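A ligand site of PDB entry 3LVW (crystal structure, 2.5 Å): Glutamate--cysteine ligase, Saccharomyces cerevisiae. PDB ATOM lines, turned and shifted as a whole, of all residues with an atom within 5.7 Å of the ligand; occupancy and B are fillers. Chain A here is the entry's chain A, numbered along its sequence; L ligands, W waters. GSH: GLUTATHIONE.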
ATOM      1  N   LEU A   4      11.393  15.926 -15.404  1.00  0.00           N
ATOM      2  CA  LEU A   4      11.756  15.548 -14.025  1.00  0.00           C
ATOM      3  C   LEU A   4      10.452  15.548 -13.169  1.00  0.00           C
ATOM      4  O   LEU A   4       9.673  16.531 -13.206  1.00  0.00           O
ATOM      5  CB  LEU A   4      12.825  16.503 -13.427  1.00  0.00           C
ATOM      6  CG  LEU A   4      14.331  16.500 -13.813  1.00  0.00           C
ATOM      7  CD1 LEU A   4      14.859  17.942 -13.786  1.00  0.00           C
ATOM      8  CD2 LEU A   4      15.213  15.559 -12.931  1.00  0.00           C
ATOM      9  N   GLU A  52      21.742  20.279 -27.076  1.00  0.00           N
ATOM     10  CA  GLU A  52      21.198  21.317 -26.241  1.00  0.00           C
ATOM     11  C   GLU A  52      21.047  22.562 -27.117  1.00  0.00           C
ATOM     12  O   GLU A  52      21.907  22.857 -27.966  1.00  0.00           O
ATOM     13  CB  GLU A  52      22.101  21.531 -24.987  1.00  0.00           C
ATOM     14  CG  GLU A  52      22.021  20.345 -23.992  1.00  0.00           C
ATOM     15  CD  GLU A  52      23.050  20.366 -22.871  1.00  0.00           C
ATOM     16  OE1 GLU A  52      24.058  21.128 -22.968  1.00  0.00           O
ATOM     17  OE2 GLU A  52      22.868  19.560 -21.870  1.00  0.00           O
ATOM     18  N   GLU A  96      16.777  21.501 -19.333  1.00  0.00           N
ATOM     19  CA  GLU A  96      18.145  21.774 -18.898  1.00  0.00           C
ATOM     20  C   GLU A  96      18.175  23.027 -17.935  1.00  0.00           C
ATOM     21  O   GLU A  96      17.111  23.647 -17.658  1.00  0.00           O
ATOM     22  CB  GLU A  96      19.058  21.939 -20.132  1.00  0.00           C
ATOM     23  CG  GLU A  96      19.938  20.723 -20.423  1.00  0.00           C
ATOM     24  CD  GLU A  96      20.807  20.272 -19.178  1.00  0.00           C
ATOM     25  OE1 GLU A  96      21.209  21.138 -18.318  1.00  0.00           O
ATOM     26  OE2 GLU A  96      21.077  19.039 -19.095  1.00  0.00           O
ATOM     27  N   TYR A  97      19.357  23.367 -17.415  1.00  0.00           N
ATOM     28  CA  TYR A  97      19.485  24.485 -16.487  1.00  0.00           C
ATOM     29  C   TYR A  97      18.766  25.732 -16.971  1.00  0.00           C
ATOM     30  O   TYR A  97      17.995  26.298 -16.214  1.00  0.00           O
ATOM     31  CB  TYR A  97      20.939  24.846 -16.160  1.00  0.00           C
ATOM     32  CG  TYR A  97      21.057  25.868 -15.046  1.00  0.00           C
ATOM     33  CD1 TYR A  97      20.822  25.492 -13.718  1.00  0.00           C
ATOM     34  CD2 TYR A  97      21.361  27.210 -15.305  1.00  0.00           C
ATOM     35  CE1 TYR A  97      20.872  26.404 -12.671  1.00  0.00           C
ATOM     36  CE2 TYR A  97      21.461  28.173 -14.244  1.00  0.00           C
ATOM     37  CZ  TYR A  97      21.209  27.752 -12.936  1.00  0.00           C
ATOM     38  OH  TYR A  97      21.243  28.642 -11.865  1.00  0.00           O
ATOM     39  N   MET A 101      16.580  27.027 -22.520  1.00  0.00           N
ATOM     40  CA  MET A 101      17.284  25.933 -23.164  1.00  0.00           C
ATOM     41  C   MET A 101      16.367  24.805 -23.491  1.00  0.00           C
ATOM     42  O   MET A 101      15.376  24.618 -22.810  1.00  0.00           O
ATOM     43  CB  MET A 101      18.367  25.416 -22.246  1.00  0.00           C
ATOM     44  CG  MET A 101      19.565  26.300 -22.240  1.00  0.00           C
ATOM     45  SD  MET A 101      20.753  25.739 -21.043  1.00  0.00           S
ATOM     46  CE  MET A 101      21.727  24.590 -22.068  1.00  0.00           C
ATOM     47  N   GLU A 103      16.782  20.475 -24.305  1.00  0.00           N
ATOM     48  CA  GLU A 103      17.604  19.291 -24.545  1.00  0.00           C
ATOM     49  C   GLU A 103      16.763  18.251 -25.288  1.00  0.00           C
ATOM     50  O   GLU A 103      15.565  18.064 -24.996  1.00  0.00           O
ATOM     51  CB  GLU A 103      18.119  18.730 -23.214  1.00  0.00           C
ATOM     52  CG  GLU A 103      19.389  17.779 -23.253  1.00  0.00           C
ATOM     53  CD  GLU A 103      19.292  16.655 -22.137  1.00  0.00           C
ATOM     54  OE1 GLU A 103      19.356  16.964 -20.880  1.00  0.00           O
ATOM     55  OE2 GLU A 103      19.069  15.447 -22.529  1.00  0.00           O
ATOM     56  N   ARG A 196      14.609  21.682  -9.027  1.00  0.00           N
ATOM     57  CA  ARG A 196      16.023  21.241  -9.001  1.00  0.00           C
ATOM     58  C   ARG A 196      16.956  22.387  -9.302  1.00  0.00           C
ATOM     59  O   ARG A 196      17.900  22.572  -8.569  1.00  0.00           O
ATOM     60  CB  ARG A 196      16.305  20.066  -9.958  1.00  0.00           C
ATOM     61  CG  ARG A 196      17.774  19.528  -9.964  1.00  0.00           C
ATOM     62  CD  ARG A 196      17.919  18.244 -10.874  1.00  0.00           C
ATOM     63  NE  ARG A 196      19.315  17.866 -11.155  1.00  0.00           N
ATOM     64  CZ  ARG A 196      20.123  17.223 -10.298  1.00  0.00           C
ATOM     65  NH1 ARG A 196      19.676  16.919  -9.092  1.00  0.00           N
ATOM     66  NH2 ARG A 196      21.369  16.900 -10.615  1.00  0.00           N
ATOM     67  N   PHE A 197      16.685  23.150 -10.357  1.00  0.00           N
ATOM     68  CA  PHE A 197      17.679  24.124 -10.836  1.00  0.00           C
ATOM     69  C   PHE A 197      17.889  25.350  -9.900  1.00  0.00           C
ATOM     70  O   PHE A 197      19.023  25.603  -9.524  1.00  0.00           O
ATOM     71  CB  PHE A 197      17.494  24.491 -12.321  1.00  0.00           C
ATOM     72  CG  PHE A 197      17.421  23.288 -13.238  1.00  0.00           C
ATOM     73  CD1 PHE A 197      18.582  22.608 -13.608  1.00  0.00           C
ATOM     74  CD2 PHE A 197      16.189  22.812 -13.706  1.00  0.00           C
ATOM     75  CE1 PHE A 197      18.520  21.507 -14.424  1.00  0.00           C
ATOM     76  CE2 PHE A 197      16.142  21.679 -14.527  1.00  0.00           C
ATOM     77  CZ  PHE A 197      17.299  21.037 -14.879  1.00  0.00           C
ATOM     78  N   LEU A 200      19.929  23.811  -6.759  1.00  0.00           N
ATOM     79  CA  LEU A 200      21.345  23.614  -6.975  1.00  0.00           C
ATOM     80  C   LEU A 200      22.062  24.966  -6.975  1.00  0.00           C
ATOM     81  O   LEU A 200      23.172  25.091  -6.450  1.00  0.00           O
ATOM     82  CB  LEU A 200      21.580  22.961  -8.334  1.00  0.00           C
ATOM     83  CG  LEU A 200      21.508  21.467  -8.456  1.00  0.00           C
ATOM     84  CD1 LEU A 200      21.727  21.184  -9.893  1.00  0.00           C
ATOM     85  CD2 LEU A 200      22.555  20.740  -7.600  1.00  0.00           C
ATOM     86  N   MET A 258      25.698  30.633 -11.794  1.00  0.00           N
ATOM     87  CA  MET A 258      25.771  29.261 -12.348  1.00  0.00           C
ATOM     88  C   MET A 258      25.373  29.201 -13.840  1.00  0.00           C
ATOM     89  O   MET A 258      25.928  28.444 -14.643  1.00  0.00           O
ATOM     90  CB  MET A 258      24.920  28.313 -11.503  1.00  0.00           C
ATOM     91  CG  MET A 258      24.885  26.882 -11.978  1.00  0.00           C
ATOM     92  SD  MET A 258      23.871  25.951 -10.809  1.00  0.00           S
ATOM     93  CE  MET A 258      23.632  24.352 -11.610  1.00  0.00           C
ATOM     94  N   GLY A 261      27.581  29.186 -16.739  1.00  0.00           N
ATOM     95  CA  GLY A 261      28.228  27.947 -17.119  1.00  0.00           C
ATOM     96  C   GLY A 261      27.216  26.920 -17.561  1.00  0.00           C
ATOM     97  O   GLY A 261      27.183  26.489 -18.703  1.00  0.00           O
ATOM     98  N   MET A 262      26.375  26.534 -16.634  1.00  0.00           N
ATOM     99  CA  MET A 262      25.360  25.542 -16.937  1.00  0.00           C
ATOM    100  C   MET A 262      24.303  26.146 -17.847  1.00  0.00           C
ATOM    101  O   MET A 262      23.380  25.432 -18.274  1.00  0.00           O
ATOM    102  CB  MET A 262      24.778  24.989 -15.657  1.00  0.00           C
ATOM    103  CG  MET A 262      25.778  24.063 -14.953  1.00  0.00           C
ATOM    104  SD  MET A 262      25.905  22.570 -15.892  1.00  0.00           S
ATOM    105  CE  MET A 262      26.624  21.501 -14.630  1.00  0.00           C
ATOM    106  N   CYS A 264      25.325  27.217 -20.674  1.00  0.00           N
ATOM    107  CA  CYS A 264      25.928  26.874 -21.940  1.00  0.00           C
ATOM    108  C   CYS A 264      25.520  25.474 -22.396  1.00  0.00           C
ATOM    109  O   CYS A 264      25.031  24.639 -21.606  1.00  0.00           O
ATOM    110  CB  CYS A 264      27.418  26.892 -21.742  1.00  0.00           C
ATOM    111  SG  CYS A 264      28.090  28.568 -21.822  1.00  0.00           S
ATOM    112  N   SER A 265      25.752  25.209 -23.675  1.00  0.00           N
ATOM    113  CA  SER A 265      25.319  23.973 -24.360  1.00  0.00           C
ATOM    114  C   SER A 265      26.512  23.179 -24.920  1.00  0.00           C
ATOM    115  O   SER A 265      27.539  23.768 -25.311  1.00  0.00           O
ATOM    116  CB  SER A 265      24.464  24.345 -25.587  1.00  0.00           C
ATOM    117  OG  SER A 265      23.124  24.661 -25.250  1.00  0.00           O
ATOM    118  N   CYS A 266      26.351  21.864 -25.030  1.00  0.00           N
ATOM    119  CA  CYS A 266      27.345  21.022 -25.639  1.00  0.00           C
ATOM    120  C   CYS A 266      26.663  19.871 -26.324  1.00  0.00           C
ATOM    121  O   CYS A 266      25.465  19.729 -26.208  1.00  0.00           O
ATOM    122  CB  CYS A 266      28.274  20.443 -24.585  1.00  0.00           C
ATOM    123  SG  CYS A 266      27.371  19.484 -23.319  1.00  0.00           S
ATOM    124  N   GLN A 268      26.712  15.683 -26.324  1.00  0.00           N
ATOM    125  CA  GLN A 268      27.199  14.582 -25.480  1.00  0.00           C
ATOM    126  C   GLN A 268      26.858  13.296 -26.154  1.00  0.00           C
ATOM    127  O   GLN A 268      25.794  13.214 -26.779  1.00  0.00           O
ATOM    128  CB  GLN A 268      26.573  14.597 -24.052  1.00  0.00           C
ATOM    129  CG  GLN A 268      27.013  15.803 -23.116  1.00  0.00           C
ATOM    130  CD  GLN A 268      26.245  15.855 -21.746  1.00  0.00           C
ATOM    131  OE1 GLN A 268      25.051  15.518 -21.644  1.00  0.00           O
ATOM    132  NE2 GLN A 268      26.943  16.310 -20.694  1.00  0.00           N
ATOM    133  N   ARG A 313      34.047  26.514 -23.617  1.00  0.00           N
ATOM    134  CA  ARG A 313      33.238  26.766 -22.440  1.00  0.00           C
ATOM    135  C   ARG A 313      33.822  26.114 -21.179  1.00  0.00           C
ATOM    136  O   ARG A 313      33.402  26.462 -20.047  1.00  0.00           O
ATOM    137  CB  ARG A 313      31.881  26.104 -22.638  1.00  0.00           C
ATOM    138  CG  ARG A 313      32.005  24.555 -22.657  1.00  0.00           C
ATOM    139  CD  ARG A 313      30.765  23.964 -23.167  1.00  0.00           C
ATOM    140  NE  ARG A 313      30.606  22.573 -22.789  1.00  0.00           N
ATOM    141  CZ  ARG A 313      31.302  21.545 -23.289  1.00  0.00           C
ATOM    142  NH1 ARG A 313      32.275  21.718 -24.199  1.00  0.00           N
ATOM    143  NH2 ARG A 313      31.029  20.319 -22.863  1.00  0.00           N
ATOM    144  N   TRP A 314      34.741  25.139 -21.361  1.00  0.00           N
ATOM    145  CA  TRP A 314      34.947  24.133 -20.325  1.00  0.00           C
ATOM    146  C   TRP A 314      35.211  24.786 -18.946  1.00  0.00           C
ATOM    147  O   TRP A 314      34.386  24.647 -18.024  1.00  0.00           O
ATOM    148  CB  TRP A 314      35.987  23.030 -20.702  1.00  0.00           C
ATOM    149  CG  TRP A 314      36.041  21.977 -19.659  1.00  0.00           C
ATOM    150  CD1 TRP A 314      36.813  21.991 -18.535  1.00  0.00           C
ATOM    151  CD2 TRP A 314      35.255  20.768 -19.589  1.00  0.00           C
ATOM    152  NE1 TRP A 314      36.560  20.883 -17.780  1.00  0.00           N
ATOM    153  CE2 TRP A 314      35.618  20.105 -18.394  1.00  0.00           C
ATOM    154  CE3 TRP A 314      34.264  20.194 -20.407  1.00  0.00           C
ATOM    155  CZ2 TRP A 314      35.023  18.891 -17.999  1.00  0.00           C
ATOM    156  CZ3 TRP A 314      33.671  18.997 -19.998  1.00  0.00           C
ATOM    157  CH2 TRP A 314      34.059  18.362 -18.806  1.00  0.00           C
ATOM    158  N   ILE A 317      32.228  26.346 -17.259  1.00  0.00           N
ATOM    159  CA  ILE A 317      31.229  25.508 -16.623  1.00  0.00           C
ATOM    160  C   ILE A 317      31.882  24.947 -15.360  1.00  0.00           C
ATOM    161  O   ILE A 317      31.190  24.794 -14.335  1.00  0.00           O
ATOM    162  CB  ILE A 317      30.700  24.405 -17.478  1.00  0.00           C
ATOM    163  CG1 ILE A 317      30.485  24.900 -18.903  1.00  0.00           C
ATOM    164  CG2 ILE A 317      29.410  23.941 -16.908  1.00  0.00           C
ATOM    165  CD1 ILE A 317      29.387  24.107 -19.668  1.00  0.00           C
ATOM    166  N   TYR A 362      33.014  19.796 -11.243  1.00  0.00           N
ATOM    167  CA  TYR A 362      32.858  19.751 -12.656  1.00  0.00           C
ATOM    168  C   TYR A 362      34.274  19.923 -13.174  1.00  0.00           C
ATOM    169  O   TYR A 362      34.797  21.038 -13.104  1.00  0.00           O
ATOM    170  CB  TYR A 362      31.955  20.899 -13.106  1.00  0.00           C
ATOM    171  CG  TYR A 362      31.666  20.887 -14.567  1.00  0.00           C
ATOM    172  CD1 TYR A 362      30.371  20.610 -15.047  1.00  0.00           C
ATOM    173  CD2 TYR A 362      32.655  21.135 -15.503  1.00  0.00           C
ATOM    174  CE1 TYR A 362      30.089  20.574 -16.389  1.00  0.00           C
ATOM    175  CE2 TYR A 362      32.380  21.128 -16.850  1.00  0.00           C
ATOM    176  CZ  TYR A 362      31.096  20.820 -17.283  1.00  0.00           C
ATOM    177  OH  TYR A 362      30.832  20.808 -18.660  1.00  0.00           O
ATOM    178  N   SER A 442      25.511  11.909 -10.633  1.00  0.00           N
ATOM    179  CA  SER A 442      25.048  12.941 -11.568  1.00  0.00           C
ATOM    180  C   SER A 442      25.549  14.402 -11.244  1.00  0.00           C
ATOM    181  O   SER A 442      25.407  15.337 -12.082  1.00  0.00           O
ATOM    182  CB  SER A 442      23.528  12.935 -11.593  1.00  0.00           C
ATOM    183  OG  SER A 442      23.142  13.723 -10.470  1.00  0.00           O
ATOM    184  N   THR A 443      26.118  14.607 -10.066  1.00  0.00           N
ATOM    185  CA  THR A 443      26.718  15.926  -9.789  1.00  0.00           C
ATOM    186  C   THR A 443      28.213  15.811  -9.604  1.00  0.00           C
ATOM    187  O   THR A 443      28.862  16.665  -8.955  1.00  0.00           O
ATOM    188  CB  THR A 443      26.048  16.646  -8.595  1.00  0.00           C
ATOM    189  OG1 THR A 443      26.199  15.823  -7.440  1.00  0.00           O
ATOM    190  CG2 THR A 443      24.516  16.866  -8.857  1.00  0.00           C
ATOM    191  N   TRP A 445      30.317  16.059 -12.640  1.00  0.00           N
ATOM    192  CA  TRP A 445      30.317  16.335 -14.092  1.00  0.00           C
ATOM    193  C   TRP A 445      31.728  16.340 -14.701  1.00  0.00           C
ATOM    194  O   TRP A 445      32.491  17.353 -14.543  1.00  0.00           O
ATOM    195  CB  TRP A 445      29.742  17.727 -14.341  1.00  0.00           C
ATOM    196  CG  TRP A 445      28.354  17.957 -13.841  1.00  0.00           C
ATOM    197  CD1 TRP A 445      27.204  17.588 -14.454  1.00  0.00           C
ATOM    198  CD2 TRP A 445      27.965  18.558 -12.609  1.00  0.00           C
ATOM    199  NE1 TRP A 445      26.136  17.931 -13.717  1.00  0.00           N
ATOM    200  CE2 TRP A 445      26.556  18.564 -12.580  1.00  0.00           C
ATOM    201  CE3 TRP A 445      28.664  19.135 -11.545  1.00  0.00           C
ATOM    202  CZ2 TRP A 445      25.794  19.136 -11.494  1.00  0.00           C
ATOM    203  CZ3 TRP A 445      27.923  19.757 -10.469  1.00  0.00           C
ATOM    204  CH2 TRP A 445      26.498  19.728 -10.458  1.00  0.00           C
ATOM    205  N   ARG A 472      31.669  13.468 -22.952  1.00  0.00           N
ATOM    206  CA  ARG A 472      31.046  14.751 -22.654  1.00  0.00           C
ATOM    207  C   ARG A 472      31.765  16.065 -23.089  1.00  0.00           C
ATOM    208  O   ARG A 472      31.224  17.130 -22.812  1.00  0.00           O
ATOM    209  CB  ARG A 472      30.779  14.861 -21.140  1.00  0.00           C
ATOM    210  CG  ARG A 472      30.030  13.705 -20.587  1.00  0.00           C
ATOM    211  CD  ARG A 472      30.168  13.647 -19.051  1.00  0.00           C
ATOM    212  NE  ARG A 472      29.714  14.904 -18.464  1.00  0.00           N
ATOM    213  CZ  ARG A 472      28.469  15.106 -18.056  1.00  0.00           C
ATOM    214  NH1 ARG A 472      27.564  14.118 -18.163  1.00  0.00           N
ATOM    215  NH2 ARG A 472      28.134  16.271 -17.525  1.00  0.00           N
HETATM  216  N1  GSH L   1      25.433  22.082 -20.439  1.00  0.00           N
HETATM  217  CA1 GSH L   1      26.431  21.146 -19.891  1.00  0.00           C
HETATM  218  C1  GSH L   1      27.764  21.181 -20.636  1.00  0.00           C
HETATM  219  O11 GSH L   1      28.683  20.462 -20.118  1.00  0.00           O
HETATM  220  O12 GSH L   1      27.937  21.918 -21.691  1.00  0.00           O
HETATM  221  CB1 GSH L   1      25.952  19.688 -19.936  1.00  0.00           C
HETATM  222  CG1 GSH L   1      24.587  19.392 -19.313  1.00  0.00           C
HETATM  223  CD1 GSH L   1      24.717  19.391 -17.799  1.00  0.00           C
HETATM  224  OE1 GSH L   1      25.752  19.085 -17.226  1.00  0.00           O
HETATM  225  N2  GSH L   1      23.599  19.746 -17.177  1.00  0.00           N
HETATM  226  CA2 GSH L   1      23.486  19.782 -15.742  1.00  0.00           C
HETATM  227  C2  GSH L   1      22.947  18.468 -15.257  1.00  0.00           C
HETATM  228  O2  GSH L   1      23.451  17.988 -14.270  1.00  0.00           O
HETATM  229  CB2 GSH L   1      22.567  20.974 -15.399  1.00  0.00           C
HETATM  230  SG2 GSH L   1      22.435  21.351 -13.629  1.00  0.00           S
HETATM  231  N3  GSH L   1      21.960  17.864 -15.926  1.00  0.00           N
HETATM  232  CA3 GSH L   1      21.299  16.609 -15.576  1.00  0.00           C
HETATM  233  C3  GSH L   1      20.245  16.979 -14.516  1.00  0.00           C
HETATM  234  O31 GSH L   1      19.956  18.205 -14.336  1.00  0.00           O
HETATM  235  O32 GSH L   1      19.680  16.076 -13.837  1.00  0.00           O
HETATM  236  O   HOH W   1      24.995  16.577 -17.468  1.00  0.00           O
HETATM  237  O   HOH W   2      29.844  18.031 -20.587  1.00  0.00           O
HETATM  238  O   HOH W   3      23.204  22.756 -18.813  1.00  0.00           O
HETATM  239  O   HOH W   4      24.625  15.044 -14.717  1.00  0.00           O
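Water W1 bridges an oxygen (OE1) of the ligand (2.6 Å) and the guanidinium group of Arg 472 (3.2 Å). Water W2 lies within hydrogen-bond range of an oxygen (O11) of the ligand, the backbone carbonyl oxygen of Arg 472, the side-chain amide nitrogen of Gln 268 and the guanidinium group of Arg 313. Water W3 lies within hydrogen-bond range of OE1 of Glu 96 (2.6 Å), O of Met 262 (2.7 Å) and N1 of the ligand (2.8 Å). Water W4 lies within hydrogen-bond range of the backbone carbonyl oxygen (O) of Ser 442, an oxygen (O2) of the ligand and the indole nitrogen (NE1) of Trp 445.
A nitrogen (N1) of the ligand is in salt-bridge range of the side-chain carboxylate (OE1) of Glu 52. The indole nitrogen (NE1) of Trp 445 is in hydrogen-bond range of an oxygen (O2) of the ligand. The side-chain carboxylate of Glu 96 is in hydrogen-bond range of a nitrogen (N2) of the ligand, at 3.0 Å. The backbone carbonyl oxygen (O) of Cys 264 is in hydrogen-bond range of a nitrogen (N1) of the ligand (2.8 Å). SG of Cys 266 is in hydrogen-bond range of O12 of the ligand. The side-chain hydroxyl (OH) of Tyr 362 lies within hydrogen-bond range of an oxygen (O11) of the ligand (2.6 Å). The guanidinium group of Arg 196 lies within salt-bridge range of an oxygen (O32) of the ligand, 3.2 Å away. The guanidinium group (NE) of Arg 313 is in salt-bridge range of an oxygen (O12) of the ligand, at 3.0 Å.
The side-chain sulfur of Met 262 sits close to an oxygen (OE1) of the ligand, at 3.7 Å. CE1 of Phe 197 touches O31 of the ligand (3.6 Å). CD1 of Leu 200 touches SG2 of the ligand, 3.8 Å away. CE of Met 258 touches SG2 of the ligand, 3.8 Å away. Ser 265 touches the ligand. Gln 268 touches the ligand. CD1 of Ile 317 touches O12 of the ligand (3.3 Å). Ser 442 touches the ligand. NH2 of Arg 472 touches OE1 of the ligand, 3.7 Å away. The nearest printed residue that does not touch the ligand is Tyr 97 (4.3 Å).
NE2 of Gln 268 sits close to NH2 of Arg 472, at 3.4 Å. The backbone carbonyl oxygen of Glu 52 lies close to the side-chain hydroxyl of Ser 265 (3.5 Å). The indole nitrogen (NE1) of Trp 445 is in hydrogen-bond range of the backbone carbonyl oxygen (O) of Ser 442 (3.2 Å). N of Cys 266 lies within hydrogen-bond range of OE1 of Glu 52, at 3.2 Å. The side-chain sulfur (SG) of Cys 266 sits close to the guanidinium group (NH2) of Arg 313 (3.8 Å). NH2 of Arg 313 is in hydrogen-bond range of O of Arg 472 (3.2 Å).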
